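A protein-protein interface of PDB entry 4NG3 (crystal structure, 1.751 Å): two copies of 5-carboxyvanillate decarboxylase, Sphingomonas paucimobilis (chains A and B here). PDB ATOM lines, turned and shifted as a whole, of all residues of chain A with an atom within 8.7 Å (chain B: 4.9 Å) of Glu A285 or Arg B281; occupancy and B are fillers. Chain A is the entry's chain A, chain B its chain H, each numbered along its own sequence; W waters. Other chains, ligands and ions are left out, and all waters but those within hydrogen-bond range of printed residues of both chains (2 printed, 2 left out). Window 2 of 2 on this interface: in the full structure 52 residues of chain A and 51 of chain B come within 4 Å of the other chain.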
ATOM      1  N   PRO A 233      -7.681   8.939 -16.278  1.00  0.00           N
ATOM      2  CA  PRO A 233      -6.819   9.346 -15.160  1.00  0.00           C
ATOM      3  C   PRO A 233      -6.315  10.800 -15.246  1.00  0.00           C
ATOM      4  O   PRO A 233      -6.078  11.417 -14.201  1.00  0.00           O
ATOM      5  CB  PRO A 233      -5.637   8.383 -15.271  1.00  0.00           C
ATOM      6  CG  PRO A 233      -6.229   7.140 -15.892  1.00  0.00           C
ATOM      7  CD  PRO A 233      -7.212   7.678 -16.894  1.00  0.00           C
ATOM      8  N   PHE A 234      -6.151  11.334 -16.452  1.00  0.00           N
ATOM      9  CA  PHE A 234      -5.681  12.715 -16.612  1.00  0.00           C
ATOM     10  C   PHE A 234      -6.751  13.738 -16.234  1.00  0.00           C
ATOM     11  O   PHE A 234      -6.421  14.841 -15.760  1.00  0.00           O
ATOM     12  CB  PHE A 234      -5.198  12.964 -18.043  1.00  0.00           C
ATOM     13  CG  PHE A 234      -4.239  14.127 -18.169  1.00  0.00           C
ATOM     14  CD1 PHE A 234      -2.977  14.060 -17.599  1.00  0.00           C
ATOM     15  CD2 PHE A 234      -4.602  15.276 -18.848  1.00  0.00           C
ATOM     16  CE1 PHE A 234      -2.079  15.124 -17.711  1.00  0.00           C
ATOM     17  CE2 PHE A 234      -3.713  16.346 -18.978  1.00  0.00           C
ATOM     18  CZ  PHE A 234      -2.450  16.269 -18.405  1.00  0.00           C
ATOM     19  N   LEU A 236      -9.195  13.474 -13.960  1.00  0.00           N
ATOM     20  CA  LEU A 236      -9.852  13.224 -12.671  1.00  0.00           C
ATOM     21  C   LEU A 236     -10.213  14.481 -11.869  1.00  0.00           C
ATOM     22  O   LEU A 236     -11.308  14.568 -11.299  1.00  0.00           O
ATOM     23  CB  LEU A 236      -9.020  12.260 -11.816  1.00  0.00           C
ATOM     24  CG  LEU A 236      -8.922  10.826 -12.349  1.00  0.00           C
ATOM     25  CD1 LEU A 236      -8.098   9.969 -11.411  1.00  0.00           C
ATOM     26  CD2 LEU A 236     -10.291  10.218 -12.569  1.00  0.00           C
ATOM     27  N   ARG A 264     -11.222   5.131  -8.987  1.00  0.00           N
ATOM     28  CA  ARG A 264     -10.246   4.358  -8.235  1.00  0.00           C
ATOM     29  C   ARG A 264     -10.859   3.109  -7.598  1.00  0.00           C
ATOM     30  O   ARG A 264     -10.187   2.082  -7.499  1.00  0.00           O
ATOM     31  CB  ARG A 264      -9.558   5.214  -7.168  1.00  0.00           C
ATOM     32  CG  ARG A 264      -8.615   6.270  -7.722  1.00  0.00           C
ATOM     33  CD  ARG A 264      -7.941   7.029  -6.567  1.00  0.00           C
ATOM     34  NE  ARG A 264      -7.546   8.373  -6.980  1.00  0.00           N
ATOM     35  CZ  ARG A 264      -8.291   9.461  -6.815  1.00  0.00           C
ATOM     36  NH1 ARG A 264      -9.472   9.388  -6.217  1.00  0.00           N
ATOM     37  NH2 ARG A 264      -7.845  10.633  -7.242  1.00  0.00           N
ATOM     38  N   ALA A 278       6.411   8.504 -18.640  1.00  0.00           N
ATOM     39  CA  ALA A 278       5.806   9.654 -17.971  1.00  0.00           C
ATOM     40  C   ALA A 278       4.330   9.408 -17.670  1.00  0.00           C
ATOM     41  O   ALA A 278       3.845   9.714 -16.577  1.00  0.00           O
ATOM     42  CB  ALA A 278       5.978  10.935 -18.803  1.00  0.00           C
ATOM     43  N   ALA A 279       3.612   8.864 -18.641  1.00  0.00           N
ATOM     44  CA  ALA A 279       2.196   8.590 -18.454  1.00  0.00           C
ATOM     45  C   ALA A 279       1.973   7.449 -17.452  1.00  0.00           C
ATOM     46  O   ALA A 279       0.996   7.441 -16.703  1.00  0.00           O
ATOM     47  CB  ALA A 279       1.530   8.283 -19.811  1.00  0.00           C
ATOM     48  N   LEU A 280       2.890   6.486 -17.437  1.00  0.00           N
ATOM     49  CA  LEU A 280       2.830   5.395 -16.465  1.00  0.00           C
ATOM     50  C   LEU A 280       3.025   5.928 -15.050  1.00  0.00           C
ATOM     51  O   LEU A 280       2.266   5.598 -14.125  1.00  0.00           O
ATOM     52  CB  LEU A 280       3.905   4.347 -16.771  1.00  0.00           C
ATOM     53  CG  LEU A 280       4.064   3.227 -15.725  1.00  0.00           C
ATOM     54  CD1 LEU A 280       2.763   2.459 -15.503  1.00  0.00           C
ATOM     55  CD2 LEU A 280       5.195   2.285 -16.110  1.00  0.00           C
ATOM     56  N   ARG A 281       4.041   6.763 -14.875  1.00  0.00           N
ATOM     57  CA  ARG A 281       4.292   7.328 -13.555  1.00  0.00           C
ATOM     58  C   ARG A 281       3.103   8.154 -13.065  1.00  0.00           C
ATOM     59  O   ARG A 281       2.683   8.011 -11.913  1.00  0.00           O
ATOM     60  CB  ARG A 281       5.564   8.172 -13.556  1.00  0.00           C
ATOM     61  CG  ARG A 281       5.776   8.972 -12.272  1.00  0.00           C
ATOM     62  CD  ARG A 281       7.231   9.408 -12.119  1.00  0.00           C
ATOM     63  NE  ARG A 281       7.894   9.537 -13.414  1.00  0.00           N
ATOM     64  CZ  ARG A 281       7.863  10.636 -14.160  1.00  0.00           C
ATOM     65  NH1 ARG A 281       7.204  11.707 -13.736  1.00  0.00           N
ATOM     66  NH2 ARG A 281       8.490  10.663 -15.329  1.00  0.00           N
ATOM     67  N   TYR A 282       2.563   8.998 -13.946  1.00  0.00           N
ATOM     68  CA  TYR A 282       1.388   9.806 -13.615  1.00  0.00           C
ATOM     69  C   TYR A 282       0.249   8.913 -13.119  1.00  0.00           C
ATOM     70  O   TYR A 282      -0.362   9.182 -12.086  1.00  0.00           O
ATOM     71  CB  TYR A 282       0.918  10.669 -14.814  1.00  0.00           C
ATOM     72  CG  TYR A 282      -0.428  11.320 -14.535  1.00  0.00           C
ATOM     73  CD1 TYR A 282      -0.505  12.554 -13.889  1.00  0.00           C
ATOM     74  CD2 TYR A 282      -1.617  10.685 -14.877  1.00  0.00           C
ATOM     75  CE1 TYR A 282      -1.731  13.133 -13.593  1.00  0.00           C
ATOM     76  CE2 TYR A 282      -2.849  11.251 -14.582  1.00  0.00           C
ATOM     77  CZ  TYR A 282      -2.899  12.473 -13.938  1.00  0.00           C
ATOM     78  OH  TYR A 282      -4.117  13.041 -13.635  1.00  0.00           O
ATOM     79  N   SER A 283      -0.026   7.846 -13.861  1.00  0.00           N
ATOM     80  CA  SER A 283      -1.150   6.955 -13.536  1.00  0.00           C
ATOM     81  C   SER A 283      -0.964   6.239 -12.211  1.00  0.00           C
ATOM     82  O   SER A 283      -1.902   6.131 -11.423  1.00  0.00           O
ATOM     83  CB  SER A 283      -1.380   5.946 -14.662  1.00  0.00           C
ATOM     84  OG  SER A 283      -1.700   6.647 -15.847  1.00  0.00           O
ATOM     85  N   ILE A 284       0.252   5.754 -11.967  1.00  0.00           N
ATOM     86  CA  ILE A 284       0.573   5.140 -10.692  1.00  0.00           C
ATOM     87  C   ILE A 284       0.372   6.135  -9.554  1.00  0.00           C
ATOM     88  O   ILE A 284      -0.204   5.790  -8.524  1.00  0.00           O
ATOM     89  CB  ILE A 284       2.006   4.586 -10.689  1.00  0.00           C
ATOM     90  CG1 ILE A 284       2.097   3.411 -11.661  1.00  0.00           C
ATOM     91  CG2 ILE A 284       2.418   4.170  -9.277  1.00  0.00           C
ATOM     92  CD1 ILE A 284       3.519   2.931 -11.938  1.00  0.00           C
ATOM     93  N   GLU A 285       0.814   7.378  -9.758  1.00  0.00           N
ATOM     94  CA  GLU A 285       0.675   8.413  -8.730  1.00  0.00           C
ATOM     95  C   GLU A 285      -0.786   8.706  -8.364  1.00  0.00           C
ATOM     96  O   GLU A 285      -1.120   8.848  -7.185  1.00  0.00           O
ATOM     97  CB  GLU A 285       1.375   9.718  -9.136  1.00  0.00           C
ATOM     98  CG  GLU A 285       1.195  10.809  -8.087  1.00  0.00           C
ATOM     99  CD  GLU A 285       1.871  12.116  -8.453  1.00  0.00           C
ATOM    100  OE1 GLU A 285       2.620  12.146  -9.456  1.00  0.00           O
ATOM    101  OE2 GLU A 285       1.651  13.120  -7.734  1.00  0.00           O
ATOM    102  N   VAL A 286      -1.656   8.801  -9.363  1.00  0.00           N
ATOM    103  CA  VAL A 286      -3.024   9.256  -9.099  1.00  0.00           C
ATOM    104  C   VAL A 286      -4.028   8.118  -8.886  1.00  0.00           C
ATOM    105  O   VAL A 286      -5.098   8.334  -8.310  1.00  0.00           O
ATOM    106  CB  VAL A 286      -3.551  10.235 -10.185  1.00  0.00           C
ATOM    107  CG1 VAL A 286      -2.587  11.434 -10.342  1.00  0.00           C
ATOM    108  CG2 VAL A 286      -3.772   9.510 -11.520  1.00  0.00           C
ATOM    109  N   LEU A 287      -3.699   6.917  -9.359  1.00  0.00           N
ATOM    110  CA  LEU A 287      -4.580   5.768  -9.149  1.00  0.00           C
ATOM    111  C   LEU A 287      -4.085   4.800  -8.084  1.00  0.00           C
ATOM    112  O   LEU A 287      -4.878   4.030  -7.533  1.00  0.00           O
ATOM    113  CB  LEU A 287      -4.791   4.982 -10.447  1.00  0.00           C
ATOM    114  CG  LEU A 287      -5.185   5.763 -11.695  1.00  0.00           C
ATOM    115  CD1 LEU A 287      -5.235   4.833 -12.878  1.00  0.00           C
ATOM    116  CD2 LEU A 287      -6.538   6.448 -11.497  1.00  0.00           C
ATOM    117  N   GLY A 288      -2.784   4.830  -7.796  1.00  0.00           N
ATOM    118  CA  GLY A 288      -2.172   3.842  -6.931  1.00  0.00           C
ATOM    119  C   GLY A 288      -1.602   2.725  -7.779  1.00  0.00           C
ATOM    120  O   GLY A 288      -2.130   2.426  -8.852  1.00  0.00           O
ATOM    121  N   PRO A 289      -0.510   2.104  -7.312  1.00  0.00           N
ATOM    122  CA  PRO A 289       0.159   1.067  -8.110  1.00  0.00           C
ATOM    123  C   PRO A 289      -0.641  -0.227  -8.278  1.00  0.00           C
ATOM    124  O   PRO A 289      -0.313  -0.996  -9.183  1.00  0.00           O
ATOM    125  CB  PRO A 289       1.448   0.797  -7.318  1.00  0.00           C
ATOM    126  CG  PRO A 289       1.121   1.215  -5.899  1.00  0.00           C
ATOM    127  CD  PRO A 289       0.233   2.425  -6.080  1.00  0.00           C
ATOM    128  N   GLU A 290      -1.644  -0.488  -7.437  1.00  0.00           N
ATOM    129  CA  GLU A 290      -2.444  -1.709  -7.584  1.00  0.00           C
ATOM    130  C   GLU A 290      -3.420  -1.618  -8.753  1.00  0.00           C
ATOM    131  O   GLU A 290      -4.029  -2.622  -9.127  1.00  0.00           O
ATOM    132  CB  GLU A 290      -3.252  -1.995  -6.316  1.00  0.00           C
ATOM    133  CG  GLU A 290      -2.419  -2.339  -5.094  1.00  0.00           C
ATOM    134  CD  GLU A 290      -3.246  -2.292  -3.829  1.00  0.00           C
ATOM    135  OE1 GLU A 290      -3.620  -1.168  -3.414  1.00  0.00           O
ATOM    136  OE2 GLU A 290      -3.527  -3.378  -3.269  1.00  0.00           O
ATOM    137  N   VAL A 292      -2.816  -0.370 -11.957  1.00  0.00           N
ATOM    138  CA  VAL A 292      -2.237  -0.288 -13.300  1.00  0.00           C
ATOM    139  C   VAL A 292      -1.646  -1.628 -13.759  1.00  0.00           C
ATOM    140  O   VAL A 292      -0.859  -2.234 -13.042  1.00  0.00           O
ATOM    141  CB  VAL A 292      -1.158   0.825 -13.388  1.00  0.00           C
ATOM    142  CG1 VAL A 292      -0.689   0.988 -14.832  1.00  0.00           C
ATOM    143  CG2 VAL A 292      -1.707   2.158 -12.860  1.00  0.00           C
ATOM    144  N   ILE A 315      10.603   2.740 -12.032  1.00  0.00           N
ATOM    145  CA  ILE A 315       9.815   2.500 -10.832  1.00  0.00           C
ATOM    146  C   ILE A 315      10.505   1.406 -10.021  1.00  0.00           C
ATOM    147  O   ILE A 315      11.281   0.623 -10.567  1.00  0.00           O
ATOM    148  CB  ILE A 315       8.368   2.064 -11.183  1.00  0.00           C
ATOM    149  CG1 ILE A 315       8.379   0.838 -12.097  1.00  0.00           C
ATOM    150  CG2 ILE A 315       7.617   3.203 -11.858  1.00  0.00           C
ATOM    151  CD1 ILE A 315       7.002   0.427 -12.623  1.00  0.00           C
ATOM    152  N   VAL A 319       6.944  -2.422  -7.349  1.00  0.00           N
ATOM    153  CA  VAL A 319       5.874  -1.828  -8.128  1.00  0.00           C
ATOM    154  C   VAL A 319       5.892  -2.348  -9.563  1.00  0.00           C
ATOM    155  O   VAL A 319       4.836  -2.599 -10.169  1.00  0.00           O
ATOM    156  CB  VAL A 319       5.988  -0.292  -8.115  1.00  0.00           C
ATOM    157  CG1 VAL A 319       4.996   0.323  -9.088  1.00  0.00           C
ATOM    158  CG2 VAL A 319       5.774   0.229  -6.704  1.00  0.00           C
ATOM    159  N   HIS B 277      -1.359  19.088  -9.219  1.00  0.00           N
ATOM    160  CA  HIS B 277       0.092  19.131  -9.276  1.00  0.00           C
ATOM    161  C   HIS B 277       0.648  17.981 -10.098  1.00  0.00           C
ATOM    162  O   HIS B 277       1.650  18.149 -10.794  1.00  0.00           O
ATOM    163  CB  HIS B 277       0.690  19.113  -7.871  1.00  0.00           C
ATOM    164  CG  HIS B 277       0.491  20.390  -7.125  1.00  0.00           C
ATOM    165  ND1 HIS B 277       0.452  20.450  -5.748  1.00  0.00           N
ATOM    166  CD2 HIS B 277       0.323  21.661  -7.565  1.00  0.00           C
ATOM    167  CE1 HIS B 277       0.272  21.706  -5.373  1.00  0.00           C
ATOM    168  NE2 HIS B 277       0.190  22.457  -6.454  1.00  0.00           N
ATOM    169  N   ALA B 278       0.015  16.808 -10.009  1.00  0.00           N
ATOM    170  CA  ALA B 278       0.459  15.662 -10.804  1.00  0.00           C
ATOM    171  C   ALA B 278       0.311  15.886 -12.317  1.00  0.00           C
ATOM    172  O   ALA B 278       1.192  15.514 -13.100  1.00  0.00           O
ATOM    173  CB  ALA B 278      -0.286  14.389 -10.376  1.00  0.00           C
ATOM    174  N   ALA B 279      -0.809  16.472 -12.730  1.00  0.00           N
ATOM    175  CA  ALA B 279      -1.049  16.715 -14.149  1.00  0.00           C
ATOM    176  C   ALA B 279      -0.154  17.854 -14.637  1.00  0.00           C
ATOM    177  O   ALA B 279       0.317  17.857 -15.778  1.00  0.00           O
ATOM    178  CB  ALA B 279      -2.536  17.032 -14.403  1.00  0.00           C
ATOM    179  N   LEU B 280       0.104  18.809 -13.752  1.00  0.00           N
ATOM    180  CA  LEU B 280       1.003  19.918 -14.071  1.00  0.00           C
ATOM    181  C   LEU B 280       2.425  19.393 -14.293  1.00  0.00           C
ATOM    182  O   LEU B 280       3.083  19.760 -15.271  1.00  0.00           O
ATOM    183  CB  LEU B 280       0.996  20.973 -12.950  1.00  0.00           C
ATOM    184  CG  LEU B 280       2.027  22.111 -13.110  1.00  0.00           C
ATOM    185  CD1 LEU B 280       1.793  22.896 -14.375  1.00  0.00           C
ATOM    186  CD2 LEU B 280       2.015  23.050 -11.889  1.00  0.00           C
ATOM    187  N   ARG B 281       2.893  18.531 -13.392  1.00  0.00           N
ATOM    188  CA  ARG B 281       4.248  17.984 -13.505  1.00  0.00           C
ATOM    189  C   ARG B 281       4.406  17.135 -14.763  1.00  0.00           C
ATOM    190  O   ARG B 281       5.420  17.232 -15.461  1.00  0.00           O
ATOM    191  CB  ARG B 281       4.634  17.188 -12.258  1.00  0.00           C
ATOM    192  CG  ARG B 281       4.896  18.072 -11.041  1.00  0.00           C
ATOM    193  CD  ARG B 281       5.531  17.308  -9.885  1.00  0.00           C
ATOM    194  NE  ARG B 281       4.626  16.305  -9.331  1.00  0.00           N
ATOM    195  CZ  ARG B 281       4.625  15.022  -9.676  1.00  0.00           C
ATOM    196  NH1 ARG B 281       5.490  14.559 -10.572  1.00  0.00           N
ATOM    197  NH2 ARG B 281       3.756  14.198  -9.121  1.00  0.00           N
ATOM    198  N   TYR B 282       3.401  16.315 -15.048  1.00  0.00           N
ATOM    199  CA  TYR B 282       3.383  15.536 -16.289  1.00  0.00           C
ATOM    200  C   TYR B 282       3.549  16.438 -17.508  1.00  0.00           C
ATOM    201  O   TYR B 282       4.398  16.196 -18.361  1.00  0.00           O
ATOM    202  CB  TYR B 282       2.099  14.696 -16.415  1.00  0.00           C
ATOM    203  CG  TYR B 282       1.989  14.039 -17.775  1.00  0.00           C
ATOM    204  CD1 TYR B 282       2.595  12.811 -18.028  1.00  0.00           C
ATOM    205  CD2 TYR B 282       1.312  14.658 -18.809  1.00  0.00           C
ATOM    206  CE1 TYR B 282       2.521  12.229 -19.286  1.00  0.00           C
ATOM    207  CE2 TYR B 282       1.227  14.094 -20.061  1.00  0.00           C
ATOM    208  CZ  TYR B 282       1.829  12.879 -20.299  1.00  0.00           C
ATOM    209  OH  TYR B 282       1.747  12.335 -21.557  1.00  0.00           O
ATOM    210  N   SER B 283       2.719  17.475 -17.589  1.00  0.00           N
ATOM    211  CA  SER B 283       2.737  18.376 -18.741  1.00  0.00           C
ATOM    212  C   SER B 283       4.083  19.069 -18.934  1.00  0.00           C
ATOM    213  O   SER B 283       4.579  19.177 -20.053  1.00  0.00           O
ATOM    214  CB  SER B 283       1.622  19.425 -18.616  1.00  0.00           C
ATOM    215  OG  SER B 283       0.353  18.793 -18.637  1.00  0.00           O
ATOM    216  N   ILE B 284       4.658  19.555 -17.839  1.00  0.00           N
ATOM    217  CA  ILE B 284       5.974  20.169 -17.893  1.00  0.00           C
ATOM    218  C   ILE B 284       6.995  19.160 -18.408  1.00  0.00           C
ATOM    219  O   ILE B 284       7.828  19.486 -19.248  1.00  0.00           O
ATOM    220  CB  ILE B 284       6.370  20.745 -16.524  1.00  0.00           C
ATOM    221  CG1 ILE B 284       5.472  21.948 -16.214  1.00  0.00           C
ATOM    222  CG2 ILE B 284       7.843  21.195 -16.530  1.00  0.00           C
ATOM    223  CD1 ILE B 284       5.545  22.435 -14.770  1.00  0.00           C
ATOM    224  N   GLU B 285       6.891  17.916 -17.945  1.00  0.00           N
ATOM    225  CA  GLU B 285       7.824  16.875 -18.362  1.00  0.00           C
ATOM    226  C   GLU B 285       7.741  16.543 -19.860  1.00  0.00           C
ATOM    227  O   GLU B 285       8.774  16.384 -20.521  1.00  0.00           O
ATOM    228  CB  GLU B 285       7.626  15.606 -17.521  1.00  0.00           C
ATOM    229  CG  GLU B 285       8.550  14.478 -17.927  1.00  0.00           C
ATOM    230  CD  GLU B 285       8.314  13.215 -17.121  1.00  0.00           C
ATOM    231  OE1 GLU B 285       7.412  13.225 -16.246  1.00  0.00           O
ATOM    232  OE2 GLU B 285       9.030  12.218 -17.368  1.00  0.00           O
ATOM    233  N   PRO B 314       4.916  21.919  -6.591  1.00  0.00           N
ATOM    234  CA  PRO B 314       6.211  21.306  -6.261  1.00  0.00           C
ATOM    235  C   PRO B 314       7.178  21.359  -7.440  1.00  0.00           C
ATOM    236  O   PRO B 314       7.589  20.324  -7.967  1.00  0.00           O
ATOM    237  CB  PRO B 314       5.839  19.853  -5.932  1.00  0.00           C
ATOM    238  CG  PRO B 314       4.602  19.591  -6.751  1.00  0.00           C
ATOM    239  CD  PRO B 314       3.844  20.914  -6.740  1.00  0.00           C
ATOM    240  N   ILE B 315       7.521  22.572  -7.855  1.00  0.00           N
ATOM    241  CA  ILE B 315       8.455  22.801  -8.952  1.00  0.00           C
ATOM    242  C   ILE B 315       9.429  23.904  -8.527  1.00  0.00           C
ATOM    243  O   ILE B 315       9.132  24.672  -7.616  1.00  0.00           O
ATOM    244  CB  ILE B 315       7.696  23.187 -10.255  1.00  0.00           C
ATOM    245  CG1 ILE B 315       6.881  24.469 -10.054  1.00  0.00           C
ATOM    246  CG2 ILE B 315       6.797  22.050 -10.697  1.00  0.00           C
ATOM    247  CD1 ILE B 315       5.930  24.780 -11.210  1.00  0.00           C
HETATM  248  O   HOH W   1       4.693  12.003 -14.997  1.00  0.00           O
HETATM  249  O   HOH W   2       2.910  13.217 -12.634  1.00  0.00           O
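The side-chain carboxylate of Glu B285 is in salt-bridge range of the guanidinium group of Arg A281 (2.6 Å).
The guanidinium group of Arg B281 is in salt-bridge range of the side-chain carboxylate of Glu A285, 2.7 Å away.
Water W1 lies within hydrogen-bond range of NH1 of Arg A281, O of Ala A278 and OE1 of Glu B285.
Water W2 bridges the backbone carbonyl oxygen of Ala B278 (2.9 Å) and the side-chain carboxylate of Glu A285 (3.4 Å).
Ala B279 touches Phe A234 (CB to CE1, 3.8 Å).
Phe A234 touches Tyr B282 (CE1 to CD2, 3.6 Å).
Phe A234 touches Ser B283 (CZ to OG, 3.8 Å).
O of Ala A278 touches CD1 of Tyr B282 (3.6 Å).
OE2 of Glu B285 touches CB of Ala A278 (3.6 Å).
N of Ala A279 touches CE1 of Tyr B282, 3.6 Å away.
Tyr A282 touches Ala B278.
CE1 of Tyr A282 touches N of Ala B279, 3.6 Å away.
OE2 of Glu A285 touches CB of Ala B278, 3.5 Å away.
Ala B278 touches Val A286.
Ala A278 touches Tyr B282, and with the chains exchanged Tyr A282 touches Ala B278.
Ala A278 touches Glu B285, and with the chains exchanged Glu A285 touches Ala B278.
Ala A279 touches Tyr B282, and with the chains exchanged Tyr A282 touches Ala B279.
Arg A281 touches Glu B285, and with the chains exchanged Glu A285 touches Arg B281.
Positions printed for both chains: 278, 279, 280, 281, 282, 283, 284, 285 and 315.
Hydrophobic or aromatic side chains of chain B that line the printed part of chain A: Ala B278, Ala B279 and Tyr B282.
Of the 20 printed residues of chain A, 7 touch a printed residue of chain B.
Hydrophobic or aromatic side chains of chain A that line the printed part of chain B: Phe A234, Ala A278, Tyr A282 and Val A286.
Among the printed residues, 12 pairs touch across the chains.
Among the printed residues, Asp or Glu carboxylates within 4 Å of a Lys or Arg side-chain nitrogen of the other chain: Arg A281 with Glu B285 (2.6 Å) and Glu A285 with Arg B281 (2.4 Å).
O of Ala B279 is in hydrogen-bond range of OG of Ser B283 (3.0 Å).
O of Pro A233 sits at hydrogen-bond distance from OH of Tyr A282, at 2.6 Å.
NE of Arg A264 lies within hydrogen-bond range of O of Val A286 (2.8 Å).
OG of Ser A283 lies within hydrogen-bond range of O of Ala A279 (2.9 Å).
Of chain A, only Glu A285 (2.4 Å) comes within 4 Å of Arg B281.
Ala B278 touches just these residues of chain A: Tyr A282, Glu A285 and Val A286.
Printed residues of chain A within 4 Å of Ala B279: Phe A234 and Tyr A282.
Printed residues of chain B within 4 Å of Ala A278: Tyr B282 (3.6 Å) and Glu B285 (3.6 Å).
Printed residues of chain B within 4 Å of Tyr A282: Ala B278 (3.5 Å) and Ala B279 (3.6 Å).
Printed residues of chain B within 4 Å of Ala A279: Tyr B282 (3.6 Å).
The nearest printed residue of chain B that does not touch Glu A285 is His B277 (5.5 Å).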
